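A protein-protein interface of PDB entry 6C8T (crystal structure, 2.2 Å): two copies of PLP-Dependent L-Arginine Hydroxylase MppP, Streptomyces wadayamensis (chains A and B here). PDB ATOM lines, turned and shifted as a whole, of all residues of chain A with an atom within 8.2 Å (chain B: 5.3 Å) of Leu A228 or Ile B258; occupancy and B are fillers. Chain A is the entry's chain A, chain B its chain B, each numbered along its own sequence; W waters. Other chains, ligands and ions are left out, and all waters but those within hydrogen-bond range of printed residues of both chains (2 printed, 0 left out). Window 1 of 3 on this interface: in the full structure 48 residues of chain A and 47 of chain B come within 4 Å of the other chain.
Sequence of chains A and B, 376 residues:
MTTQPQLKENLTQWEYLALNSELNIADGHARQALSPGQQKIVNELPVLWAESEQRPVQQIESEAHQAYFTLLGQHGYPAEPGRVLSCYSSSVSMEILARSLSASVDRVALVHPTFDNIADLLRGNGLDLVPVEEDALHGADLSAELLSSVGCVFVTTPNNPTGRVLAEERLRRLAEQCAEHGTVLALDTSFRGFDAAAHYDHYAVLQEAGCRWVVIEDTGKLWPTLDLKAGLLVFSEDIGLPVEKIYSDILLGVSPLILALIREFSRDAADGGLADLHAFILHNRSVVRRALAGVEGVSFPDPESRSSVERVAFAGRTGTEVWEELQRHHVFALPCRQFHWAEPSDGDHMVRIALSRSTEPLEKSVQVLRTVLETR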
ATOM      1  N   HIS A  29       6.441   9.712  12.374  1.00  0.00           N
ATOM      2  CA  HIS A  29       6.680   9.185  11.048  1.00  0.00           C
ATOM      3  C   HIS A  29       6.465   7.671  11.056  1.00  0.00           C
ATOM      4  O   HIS A  29       6.548   6.997  12.091  1.00  0.00           O
ATOM      5  CB  HIS A  29       8.108   9.506  10.560  1.00  0.00           C
ATOM      6  CG  HIS A  29       8.372  10.961  10.266  1.00  0.00           C
ATOM      7  ND1 HIS A  29       7.380  11.914  10.192  1.00  0.00           N
ATOM      8  CD2 HIS A  29       9.533  11.614   9.996  1.00  0.00           C
ATOM      9  CE1 HIS A  29       7.916  13.092   9.910  1.00  0.00           C
ATOM     10  NE2 HIS A  29       9.221  12.937   9.782  1.00  0.00           N
ATOM     11  N   ALA A  30       6.140   7.143   9.891  1.00  0.00           N
ATOM     12  CA  ALA A  30       5.908   5.719   9.736  1.00  0.00           C
ATOM     13  C   ALA A  30       7.255   4.999   9.666  1.00  0.00           C
ATOM     14  O   ALA A  30       8.053   5.239   8.750  1.00  0.00           O
ATOM     15  CB  ALA A  30       5.071   5.460   8.484  1.00  0.00           C
ATOM     16  N   VAL A  42       8.887  -1.364  -3.722  1.00  0.00           N
ATOM     17  CA  VAL A  42      10.279  -0.954  -3.534  1.00  0.00           C
ATOM     18  C   VAL A  42      11.185  -1.763  -4.458  1.00  0.00           C
ATOM     19  O   VAL A  42      12.103  -1.218  -5.084  1.00  0.00           O
ATOM     20  CB  VAL A  42      10.691  -1.085  -2.048  1.00  0.00           C
ATOM     21  CG1 VAL A  42      12.220  -1.037  -1.858  1.00  0.00           C
ATOM     22  CG2 VAL A  42      10.019   0.019  -1.210  1.00  0.00           C
ATOM     23  N   LEU A  45      11.588  -0.217  -7.874  1.00  0.00           N
ATOM     24  CA  LEU A  45      12.079   1.151  -7.985  1.00  0.00           C
ATOM     25  C   LEU A  45      12.825   1.431  -9.278  1.00  0.00           C
ATOM     26  O   LEU A  45      12.583   2.493  -9.874  1.00  0.00           O
ATOM     27  CB  LEU A  45      12.959   1.451  -6.771  1.00  0.00           C
ATOM     28  CG  LEU A  45      12.129   2.004  -5.625  1.00  0.00           C
ATOM     29  CD1 LEU A  45      12.930   1.947  -4.347  1.00  0.00           C
ATOM     30  CD2 LEU A  45      11.729   3.419  -5.971  1.00  0.00           C
ATOM     31  N   TYR A  88       7.762  19.380  -0.992  1.00  0.00           N
ATOM     32  CA  TYR A  88       8.637  18.356  -0.426  1.00  0.00           C
ATOM     33  C   TYR A  88       8.064  17.766   0.859  1.00  0.00           C
ATOM     34  O   TYR A  88       8.387  16.636   1.219  1.00  0.00           O
ATOM     35  CB  TYR A  88      10.000  18.942  -0.122  1.00  0.00           C
ATOM     36  CG  TYR A  88      10.729  19.523  -1.304  1.00  0.00           C
ATOM     37  CD1 TYR A  88      11.059  18.736  -2.402  1.00  0.00           C
ATOM     38  CD2 TYR A  88      11.140  20.846  -1.295  1.00  0.00           C
ATOM     39  CE1 TYR A  88      11.770  19.249  -3.470  1.00  0.00           C
ATOM     40  CE2 TYR A  88      11.858  21.370  -2.360  1.00  0.00           C
ATOM     41  CZ  TYR A  88      12.181  20.552  -3.443  1.00  0.00           C
ATOM     42  OH  TYR A  88      12.861  21.067  -4.510  1.00  0.00           O
ATOM     43  N   ASP A 218      -1.058  15.364   3.254  1.00  0.00           N
ATOM     44  CA  ASP A 218       0.279  14.827   3.478  1.00  0.00           C
ATOM     45  C   ASP A 218       0.269  13.318   3.293  1.00  0.00           C
ATOM     46  O   ASP A 218      -0.576  12.638   3.877  1.00  0.00           O
ATOM     47  CB  ASP A 218       0.722  15.165   4.894  1.00  0.00           C
ATOM     48  CG  ASP A 218       2.152  14.810   5.169  1.00  0.00           C
ATOM     49  OD1 ASP A 218       2.890  14.463   4.213  1.00  0.00           O
ATOM     50  OD2 ASP A 218       2.540  14.887   6.357  1.00  0.00           O
ATOM     51  N   THR A 219       1.227  12.791   2.524  1.00  0.00           N
ATOM     52  CA  THR A 219       1.344  11.352   2.353  1.00  0.00           C
ATOM     53  C   THR A 219       2.317  10.740   3.336  1.00  0.00           C
ATOM     54  O   THR A 219       2.374   9.512   3.442  1.00  0.00           O
ATOM     55  CB  THR A 219       1.801  11.005   0.934  1.00  0.00           C
ATOM     56  OG1 THR A 219       3.198  11.330   0.780  1.00  0.00           O
ATOM     57  CG2 THR A 219       0.966  11.788  -0.085  1.00  0.00           C
ATOM     58  N   GLY A 220       3.051  11.566   4.077  1.00  0.00           N
ATOM     59  CA  GLY A 220       4.198  11.066   4.828  1.00  0.00           C
ATOM     60  C   GLY A 220       3.861  10.167   6.015  1.00  0.00           C
ATOM     61  O   GLY A 220       4.599   9.214   6.287  1.00  0.00           O
ATOM     62  N   TRP A 223       2.672   5.715   5.374  1.00  0.00           N
ATOM     63  CA  TRP A 223       3.407   4.549   4.910  1.00  0.00           C
ATOM     64  C   TRP A 223       4.884   4.673   5.221  1.00  0.00           C
ATOM     65  O   TRP A 223       5.444   5.771   5.176  1.00  0.00           O
ATOM     66  CB  TRP A 223       3.256   4.344   3.401  1.00  0.00           C
ATOM     67  CG  TRP A 223       1.858   4.337   2.974  1.00  0.00           C
ATOM     68  CD1 TRP A 223       0.880   3.485   3.389  1.00  0.00           C
ATOM     69  CD2 TRP A 223       1.255   5.213   2.017  1.00  0.00           C
ATOM     70  NE1 TRP A 223      -0.298   3.773   2.747  1.00  0.00           N
ATOM     71  CE2 TRP A 223      -0.096   4.837   1.904  1.00  0.00           C
ATOM     72  CE3 TRP A 223       1.731   6.277   1.239  1.00  0.00           C
ATOM     73  CZ2 TRP A 223      -0.989   5.493   1.057  1.00  0.00           C
ATOM     74  CZ3 TRP A 223       0.837   6.928   0.397  1.00  0.00           C
ATOM     75  CH2 TRP A 223      -0.505   6.527   0.312  1.00  0.00           C
ATOM     76  N   PRO A 224       5.547   3.558   5.482  1.00  0.00           N
ATOM     77  CA  PRO A 224       6.982   3.597   5.810  1.00  0.00           C
ATOM     78  C   PRO A 224       7.854   3.716   4.567  1.00  0.00           C
ATOM     79  O   PRO A 224       8.425   2.754   4.055  1.00  0.00           O
ATOM     80  CB  PRO A 224       7.193   2.269   6.534  1.00  0.00           C
ATOM     81  CG  PRO A 224       6.213   1.358   5.887  1.00  0.00           C
ATOM     82  CD  PRO A 224       5.002   2.196   5.557  1.00  0.00           C
ATOM     83  N   THR A 225       7.987   4.947   4.079  1.00  0.00           N
ATOM     84  CA  THR A 225       8.680   5.206   2.818  1.00  0.00           C
ATOM     85  C   THR A 225      10.018   5.907   3.011  1.00  0.00           C
ATOM     86  O   THR A 225      10.486   6.603   2.101  1.00  0.00           O
ATOM     87  CB  THR A 225       7.803   6.054   1.909  1.00  0.00           C
ATOM     88  OG1 THR A 225       7.491   7.279   2.584  1.00  0.00           O
ATOM     89  CG2 THR A 225       6.540   5.282   1.524  1.00  0.00           C
ATOM     90  N   LEU A 226      10.622   5.772   4.183  1.00  0.00           N
ATOM     91  CA  LEU A 226      11.893   6.422   4.455  1.00  0.00           C
ATOM     92  C   LEU A 226      11.791   7.920   4.194  1.00  0.00           C
ATOM     93  O   LEU A 226      12.685   8.529   3.605  1.00  0.00           O
ATOM     94  CB  LEU A 226      13.016   5.792   3.615  1.00  0.00           C
ATOM     95  CG  LEU A 226      13.198   4.291   3.733  1.00  0.00           C
ATOM     96  CD1 LEU A 226      14.272   3.798   2.747  1.00  0.00           C
ATOM     97  CD2 LEU A 226      13.562   3.939   5.187  1.00  0.00           C
ATOM     98  N   ASP A 227      10.688   8.518   4.635  1.00  0.00           N
ATOM     99  CA  ASP A 227      10.439   9.954   4.537  1.00  0.00           C
ATOM    100  C   ASP A 227      10.333  10.451   3.101  1.00  0.00           C
ATOM    101  O   ASP A 227      10.414  11.659   2.874  1.00  0.00           O
ATOM    102  CB  ASP A 227      11.519  10.771   5.260  1.00  0.00           C
ATOM    103  CG  ASP A 227      11.229  10.925   6.707  1.00  0.00           C
ATOM    104  OD1 ASP A 227      11.008   9.888   7.385  1.00  0.00           O
ATOM    105  OD2 ASP A 227      11.205  12.079   7.167  1.00  0.00           O
ATOM    106  N   LEU A 228      10.166   9.554   2.131  1.00  0.00           N
ATOM    107  CA  LEU A 228       9.825   9.948   0.763  1.00  0.00           C
ATOM    108  C   LEU A 228       8.329  10.238   0.685  1.00  0.00           C
ATOM    109  O   LEU A 228       7.493   9.337   0.876  1.00  0.00           O
ATOM    110  CB  LEU A 228      10.212   8.856  -0.230  1.00  0.00           C
ATOM    111  CG  LEU A 228      11.710   8.538  -0.255  1.00  0.00           C
ATOM    112  CD1 LEU A 228      11.946   7.282  -1.073  1.00  0.00           C
ATOM    113  CD2 LEU A 228      12.513   9.716  -0.818  1.00  0.00           C
ATOM    114  N   LYS A 229       7.984  11.479   0.359  1.00  0.00           N
ATOM    115  CA  LYS A 229       6.646  11.968   0.668  1.00  0.00           C
ATOM    116  C   LYS A 229       6.415  13.266  -0.078  1.00  0.00           C
ATOM    117  O   LYS A 229       7.339  13.866  -0.614  1.00  0.00           O
ATOM    118  CB  LYS A 229       6.485  12.203   2.176  1.00  0.00           C
ATOM    119  CG  LYS A 229       7.396  13.306   2.692  1.00  0.00           C
ATOM    120  CD  LYS A 229       7.470  13.418   4.244  1.00  0.00           C
ATOM    121  CE  LYS A 229       8.562  14.419   4.655  1.00  0.00           C
ATOM    122  NZ  LYS A 229       8.817  14.442   6.139  1.00  0.00           N
ATOM    123  N   ALA A 230       5.172  13.732  -0.032  1.00  0.00           N
ATOM    124  CA  ALA A 230       4.864  15.076  -0.468  1.00  0.00           C
ATOM    125  C   ALA A 230       3.823  15.688   0.444  1.00  0.00           C
ATOM    126  O   ALA A 230       2.919  14.995   0.930  1.00  0.00           O
ATOM    127  CB  ALA A 230       4.347  15.088  -1.915  1.00  0.00           C
ATOM    128  N   GLY A 231       3.950  16.991   0.680  1.00  0.00           N
ATOM    129  CA  GLY A 231       2.836  17.767   1.189  1.00  0.00           C
ATOM    130  C   GLY A 231       2.062  18.288  -0.013  1.00  0.00           C
ATOM    131  O   GLY A 231       2.643  18.667  -1.023  1.00  0.00           O
ATOM    132  N   SER A 255      10.208  15.367  -6.968  1.00  0.00           N
ATOM    133  CA  SER A 255      10.705  14.265  -7.782  1.00  0.00           C
ATOM    134  C   SER A 255       9.558  13.459  -8.395  1.00  0.00           C
ATOM    135  O   SER A 255       8.646  13.026  -7.671  1.00  0.00           O
ATOM    136  CB  SER A 255      11.579  13.320  -6.950  1.00  0.00           C
ATOM    137  OG  SER A 255      11.947  12.161  -7.714  1.00  0.00           O
ATOM    138  N   LEU A 257       9.823  10.462  -9.188  1.00  0.00           N
ATOM    139  CA  LEU A 257       9.943   9.148  -8.560  1.00  0.00           C
ATOM    140  C   LEU A 257       9.121   9.093  -7.277  1.00  0.00           C
ATOM    141  O   LEU A 257       8.431   8.100  -7.008  1.00  0.00           O
ATOM    142  CB  LEU A 257      11.407   8.833  -8.261  1.00  0.00           C
ATOM    143  CG  LEU A 257      11.652   7.416  -7.742  1.00  0.00           C
ATOM    144  CD1 LEU A 257      11.372   6.404  -8.844  1.00  0.00           C
ATOM    145  CD2 LEU A 257      13.060   7.245  -7.276  1.00  0.00           C
ATOM    146  N   ILE A 258       9.138  10.171  -6.503  1.00  0.00           N
ATOM    147  CA  ILE A 258       8.339  10.201  -5.281  1.00  0.00           C
ATOM    148  C   ILE A 258       6.861  10.214  -5.637  1.00  0.00           C
ATOM    149  O   ILE A 258       6.045   9.507  -5.029  1.00  0.00           O
ATOM    150  CB  ILE A 258       8.746  11.418  -4.431  1.00  0.00           C
ATOM    151  CG1 ILE A 258      10.171  11.186  -3.927  1.00  0.00           C
ATOM    152  CG2 ILE A 258       7.727  11.637  -3.276  1.00  0.00           C
ATOM    153  CD1 ILE A 258      10.754  12.327  -3.088  1.00  0.00           C
ATOM    154  N   LEU A 259       6.497  11.013  -6.638  1.00  0.00           N
ATOM    155  CA  LEU A 259       5.122  11.018  -7.126  1.00  0.00           C
ATOM    156  C   LEU A 259       4.699   9.621  -7.584  1.00  0.00           C
ATOM    157  O   LEU A 259       3.596   9.157  -7.279  1.00  0.00           O
ATOM    158  CB  LEU A 259       5.002  12.014  -8.265  1.00  0.00           C
ATOM    159  CG  LEU A 259       4.511  13.460  -8.137  1.00  0.00           C
ATOM    160  CD1 LEU A 259       4.069  13.887  -6.784  1.00  0.00           C
ATOM    161  CD2 LEU A 259       5.482  14.444  -8.721  1.00  0.00           C
ATOM    162  N   LEU A 261       5.914   6.767  -6.585  1.00  0.00           N
ATOM    163  CA  LEU A 261       5.835   5.993  -5.350  1.00  0.00           C
ATOM    164  C   LEU A 261       4.526   6.221  -4.612  1.00  0.00           C
ATOM    165  O   LEU A 261       3.887   5.274  -4.135  1.00  0.00           O
ATOM    166  CB  LEU A 261       7.010   6.397  -4.467  1.00  0.00           C
ATOM    167  CG  LEU A 261       7.557   5.410  -3.453  1.00  0.00           C
ATOM    168  CD1 LEU A 261       8.156   4.218  -4.155  1.00  0.00           C
ATOM    169  CD2 LEU A 261       8.601   6.096  -2.619  1.00  0.00           C
ATOM    170  N   ILE A 262       4.160   7.488  -4.430  1.00  0.00           N
ATOM    171  CA  ILE A 262       2.879   7.834  -3.826  1.00  0.00           C
ATOM    172  C   ILE A 262       1.753   7.166  -4.601  1.00  0.00           C
ATOM    173  O   ILE A 262       0.841   6.571  -4.019  1.00  0.00           O
ATOM    174  CB  ILE A 262       2.734   9.370  -3.784  1.00  0.00           C
ATOM    175  CG1 ILE A 262       3.791   9.961  -2.827  1.00  0.00           C
ATOM    176  CG2 ILE A 262       1.323   9.804  -3.420  1.00  0.00           C
ATOM    177  CD1 ILE A 262       3.886  11.469  -2.847  1.00  0.00           C
ATOM    178  N   PHE A 265       1.885   3.387  -3.768  1.00  0.00           N
ATOM    179  CA  PHE A 265       1.457   3.075  -2.404  1.00  0.00           C
ATOM    180  C   PHE A 265      -0.029   3.352  -2.222  1.00  0.00           C
ATOM    181  O   PHE A 265      -0.725   2.609  -1.513  1.00  0.00           O
ATOM    182  CB  PHE A 265       2.287   3.867  -1.388  1.00  0.00           C
ATOM    183  CG  PHE A 265       3.569   3.194  -0.990  1.00  0.00           C
ATOM    184  CD1 PHE A 265       4.636   3.105  -1.873  1.00  0.00           C
ATOM    185  CD2 PHE A 265       3.727   2.690   0.270  1.00  0.00           C
ATOM    186  CE1 PHE A 265       5.811   2.495  -1.493  1.00  0.00           C
ATOM    187  CE2 PHE A 265       4.899   2.069   0.651  1.00  0.00           C
ATOM    188  CZ  PHE A 265       5.936   1.974  -0.222  1.00  0.00           C
ATOM    189  N   TRP B  49      17.622   0.823  -0.133  1.00  0.00           N
ATOM    190  CA  TRP B  49      16.445   0.965   0.719  1.00  0.00           C
ATOM    191  C   TRP B  49      16.607   0.156   1.999  1.00  0.00           C
ATOM    192  O   TRP B  49      16.388   0.666   3.101  1.00  0.00           O
ATOM    193  CB  TRP B  49      15.205   0.513  -0.042  1.00  0.00           C
ATOM    194  CG  TRP B  49      13.931   0.830   0.666  1.00  0.00           C
ATOM    195  CD1 TRP B  49      13.482   0.253   1.804  1.00  0.00           C
ATOM    196  CD2 TRP B  49      12.952   1.801   0.291  1.00  0.00           C
ATOM    197  NE1 TRP B  49      12.292   0.812   2.179  1.00  0.00           N
ATOM    198  CE2 TRP B  49      11.941   1.766   1.261  1.00  0.00           C
ATOM    199  CE3 TRP B  49      12.838   2.701  -0.766  1.00  0.00           C
ATOM    200  CZ2 TRP B  49      10.810   2.585   1.197  1.00  0.00           C
ATOM    201  CZ3 TRP B  49      11.730   3.519  -0.830  1.00  0.00           C
ATOM    202  CH2 TRP B  49      10.723   3.459   0.153  1.00  0.00           C
ATOM    203  N   LEU B 228      16.093  14.092  -6.908  1.00  0.00           N
ATOM    204  CA  LEU B 228      16.434  13.595  -5.575  1.00  0.00           C
ATOM    205  C   LEU B 228      17.796  14.154  -5.176  1.00  0.00           C
ATOM    206  O   LEU B 228      18.813  13.861  -5.810  1.00  0.00           O
ATOM    207  CB  LEU B 228      16.438  12.065  -5.547  1.00  0.00           C
ATOM    208  CG  LEU B 228      15.131  11.393  -6.000  1.00  0.00           C
ATOM    209  CD1 LEU B 228      15.363   9.923  -6.223  1.00  0.00           C
ATOM    210  CD2 LEU B 228      14.002  11.609  -5.015  1.00  0.00           C
ATOM    211  N   LYS B 229      17.807  14.939  -4.107  1.00  0.00           N
ATOM    212  CA  LYS B 229      18.883  15.878  -3.828  1.00  0.00           C
ATOM    213  C   LYS B 229      18.769  16.322  -2.378  1.00  0.00           C
ATOM    214  O   LYS B 229      17.756  16.094  -1.709  1.00  0.00           O
ATOM    215  CB  LYS B 229      18.804  17.103  -4.748  1.00  0.00           C
ATOM    216  CG  LYS B 229      17.477  17.868  -4.572  1.00  0.00           C
ATOM    217  CD  LYS B 229      17.144  18.833  -5.720  1.00  0.00           C
ATOM    218  CE  LYS B 229      15.776  19.497  -5.504  1.00  0.00           C
ATOM    219  NZ  LYS B 229      15.382  20.431  -6.632  1.00  0.00           N
ATOM    220  N   ALA B 230      19.812  16.992  -1.913  1.00  0.00           N
ATOM    221  CA  ALA B 230      19.742  17.740  -0.667  1.00  0.00           C
ATOM    222  C   ALA B 230      20.429  19.077  -0.851  1.00  0.00           C
ATOM    223  O   ALA B 230      21.433  19.193  -1.565  1.00  0.00           O
ATOM    224  CB  ALA B 230      20.387  17.004   0.492  1.00  0.00           C
ATOM    225  N   SER B 255      15.381  12.093   3.788  1.00  0.00           N
ATOM    226  CA  SER B 255      15.327  10.643   3.634  1.00  0.00           C
ATOM    227  C   SER B 255      16.725  10.031   3.686  1.00  0.00           C
ATOM    228  O   SER B 255      17.632  10.492   2.978  1.00  0.00           O
ATOM    229  CB  SER B 255      14.661  10.260   2.315  1.00  0.00           C
ATOM    230  OG  SER B 255      14.844   8.875   2.046  1.00  0.00           O
ATOM    231  N   PRO B 256      16.937   8.980   4.476  1.00  0.00           N
ATOM    232  CA  PRO B 256      18.210   8.257   4.371  1.00  0.00           C
ATOM    233  C   PRO B 256      18.457   7.672   2.997  1.00  0.00           C
ATOM    234  O   PRO B 256      19.622   7.532   2.607  1.00  0.00           O
ATOM    235  CB  PRO B 256      18.084   7.159   5.437  1.00  0.00           C
ATOM    236  CG  PRO B 256      16.641   7.056   5.715  1.00  0.00           C
ATOM    237  CD  PRO B 256      16.077   8.421   5.521  1.00  0.00           C
ATOM    238  N   LEU B 257      17.412   7.347   2.234  1.00  0.00           N
ATOM    239  CA  LEU B 257      17.646   6.799   0.905  1.00  0.00           C
ATOM    240  C   LEU B 257      18.277   7.840  -0.004  1.00  0.00           C
ATOM    241  O   LEU B 257      19.175   7.521  -0.789  1.00  0.00           O
ATOM    242  CB  LEU B 257      16.343   6.282   0.293  1.00  0.00           C
ATOM    243  CG  LEU B 257      16.532   5.496  -1.017  1.00  0.00           C
ATOM    244  CD1 LEU B 257      17.217   4.174  -0.746  1.00  0.00           C
ATOM    245  CD2 LEU B 257      15.207   5.246  -1.675  1.00  0.00           C
ATOM    246  N   ILE B 258      17.831   9.093   0.102  1.00  0.00           N
ATOM    247  CA  ILE B 258      18.432  10.162  -0.678  1.00  0.00           C
ATOM    248  C   ILE B 258      19.866  10.397  -0.230  1.00  0.00           C
ATOM    249  O   ILE B 258      20.761  10.619  -1.054  1.00  0.00           O
ATOM    250  CB  ILE B 258      17.575  11.437  -0.578  1.00  0.00           C
ATOM    251  CG1 ILE B 258      16.219  11.217  -1.269  1.00  0.00           C
ATOM    252  CG2 ILE B 258      18.307  12.639  -1.179  1.00  0.00           C
ATOM    253  CD1 ILE B 258      15.242  12.409  -1.149  1.00  0.00           C
ATOM    254  N   LEU B 259      20.124  10.341   1.075  1.00  0.00           N
ATOM    255  CA  LEU B 259      21.496  10.554   1.515  1.00  0.00           C
ATOM    256  C   LEU B 259      22.410   9.454   0.986  1.00  0.00           C
ATOM    257  O   LEU B 259      23.544   9.726   0.573  1.00  0.00           O
ATOM    258  CB  LEU B 259      21.554  10.642   3.039  1.00  0.00           C
ATOM    259  CG  LEU B 259      20.918  11.903   3.620  1.00  0.00           C
ATOM    260  CD1 LEU B 259      20.632  11.702   5.090  1.00  0.00           C
ATOM    261  CD2 LEU B 259      21.832  13.143   3.370  1.00  0.00           C
ATOM    262  N   ALA B 260      21.919   8.208   0.977  1.00  0.00           N
ATOM    263  CA  ALA B 260      22.693   7.092   0.438  1.00  0.00           C
ATOM    264  C   ALA B 260      22.901   7.253  -1.061  1.00  0.00           C
ATOM    265  O   ALA B 260      23.977   6.959  -1.587  1.00  0.00           O
ATOM    266  CB  ALA B 260      21.977   5.774   0.730  1.00  0.00           C
ATOM    267  N   LEU B 261      21.882   7.733  -1.762  1.00  0.00           N
ATOM    268  CA  LEU B 261      22.033   8.012  -3.182  1.00  0.00           C
ATOM    269  C   LEU B 261      23.103   9.073  -3.420  1.00  0.00           C
ATOM    270  O   LEU B 261      23.948   8.932  -4.321  1.00  0.00           O
ATOM    271  CB  LEU B 261      20.691   8.447  -3.746  1.00  0.00           C
ATOM    272  CG  LEU B 261      20.268   7.896  -5.095  1.00  0.00           C
ATOM    273  CD1 LEU B 261      20.182   6.390  -5.048  1.00  0.00           C
ATOM    274  CD2 LEU B 261      18.919   8.495  -5.457  1.00  0.00           C
ATOM    275  N   ILE B 262      23.103  10.131  -2.605  1.00  0.00           N
ATOM    276  CA  ILE B 262      24.161  11.139  -2.711  1.00  0.00           C
ATOM    277  C   ILE B 262      25.518  10.513  -2.455  1.00  0.00           C
ATOM    278  O   ILE B 262      26.493  10.801  -3.160  1.00  0.00           O
ATOM    279  CB  ILE B 262      23.902  12.309  -1.747  1.00  0.00           C
ATOM    280  CG1 ILE B 262      22.716  13.101  -2.266  1.00  0.00           C
ATOM    281  CG2 ILE B 262      25.155  13.187  -1.588  1.00  0.00           C
ATOM    282  CD1 ILE B 262      22.205  14.135  -1.299  1.00  0.00           C
ATOM    283  N   ARG B 263      25.616   9.677  -1.425  1.00  0.00           N
ATOM    284  CA  ARG B 263      26.877   9.003  -1.157  1.00  0.00           C
ATOM    285  C   ARG B 263      27.345   8.213  -2.386  1.00  0.00           C
ATOM    286  O   ARG B 263      28.510   8.299  -2.788  1.00  0.00           O
ATOM    287  CB  ARG B 263      26.729   8.089   0.052  1.00  0.00           C
ATOM    288  CG  ARG B 263      28.002   7.285   0.393  1.00  0.00           C
ATOM    289  CD  ARG B 263      27.657   6.206   1.381  1.00  0.00           C
ATOM    290  NE  ARG B 263      26.866   5.141   0.756  1.00  0.00           N
ATOM    291  CZ  ARG B 263      26.090   4.303   1.431  1.00  0.00           C
ATOM    292  NH1 ARG B 263      25.991   4.419   2.755  1.00  0.00           N
ATOM    293  NH2 ARG B 263      25.412   3.352   0.786  1.00  0.00           N
HETATM  294  O   HOH W   1      10.617   1.397   5.055  1.00  0.00           O
HETATM  295  O   HOH W   2      12.611  20.279  -7.646  1.00  0.00           O
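The side-chain hydroxyl (OH) of Tyr A88 is in hydrogen-bond range of the side-chain amino group (NZ) of Lys B229 (3.4 Å). The backbone carbonyl oxygen (O) of Leu A226 lies within hydrogen-bond range of the side-chain hydroxyl (OG) of Ser B255 (2.7 Å).
OG1 of Thr A225 is in hydrogen-bond range of O of Leu A228 (2.7 Å). OG of Ser A255 lies within hydrogen-bond range of N of Leu A257 (3.1 Å). The backbone NH of Leu B257 is in hydrogen-bond range of the side-chain hydroxyl of Ser B255 (3.0 Å).
Among the printed residues, pairs that only touch across the chains: Val A42 with Trp B49 (3.6 Å), Leu A45 with Trp B49 (3.7 Å), Pro A224 with Trp B49 (3.7 Å), Thr A225 with Trp B49 (3.7 Å), Leu A226 with Trp B49 (3.4 Å), Leu A226 with Pro B256 (3.9 Å), Leu A228 with Trp B49 (3.8 Å), Leu A228 with Ser B255 (3.8 Å), Leu A228 with Leu B257 (3.9 Å), Leu A228 with Ile B258 (3.8 Å), Ser A255 with Leu B228 (3.4 Å), Leu A257 with Leu B228 (3.7 Å) and Ile A258 with Leu B228 (3.8 Å).
Of the printed residues of chain B, Pro A224 touches Trp B49 (3.7 Å). Printed residues of chain B within 4 Å of Thr A225: Trp B49 (3.7 Å). Printed residues of chain B within 4 Å of Leu A228: Trp B49, Ser B255, Leu B257 and Ile B258. Of the printed residues of chain A, Ser B255 touches Leu A226 and Leu A228. Of chain A, only Leu A228 (3.8 Å) comes within 4 Å of Ile B258. Leu B259 touches none of the printed residues of chain A. The nearest residue of chain B that does not touch Leu A228 is Leu B228 (4.8 Å). The nearest printed residue of chain B that does not touch Thr A225 is Ser B255 (4.9 Å).
Hydrophobic or aromatic side chains of chain B that line the printed part of chain A: Trp B49, Leu B228, Pro B256, Leu B257 and Ile B258. Of the 24 printed residues of chain A, 10 touch a printed residue of chain B. Printed residues of chain A that touch a printed residue of chain B: Val A42, Leu A45, Tyr A88, Pro A224, Thr A225, Leu A226, Leu A228, Ser A255, Leu A257 and Ile A258. Among the printed residues, 15 pairs touch across the chains.
Leu A228 touches Ser B255, and with the chains exchanged Ser A255 touches Leu B228. Leu A228 touches Leu B257, and with the chains exchanged Leu A257 touches Leu B228. Leu A228 touches Ile B258, and with the chains exchanged Ile A258 touches Leu B228. 9 positions are printed for both chains. Of the 15 pairs that touch across the chains among the printed residues, 6 have their exchanged pair printed and touching as well.
Water W1 bridges O of Pro A224 and NE1 of Trp B49. Water W2 lies within hydrogen-bond range of the side-chain amino group of Lys B229 (3.0 Å) and the side-chain hydroxyl of Tyr A88 (3.2 Å).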
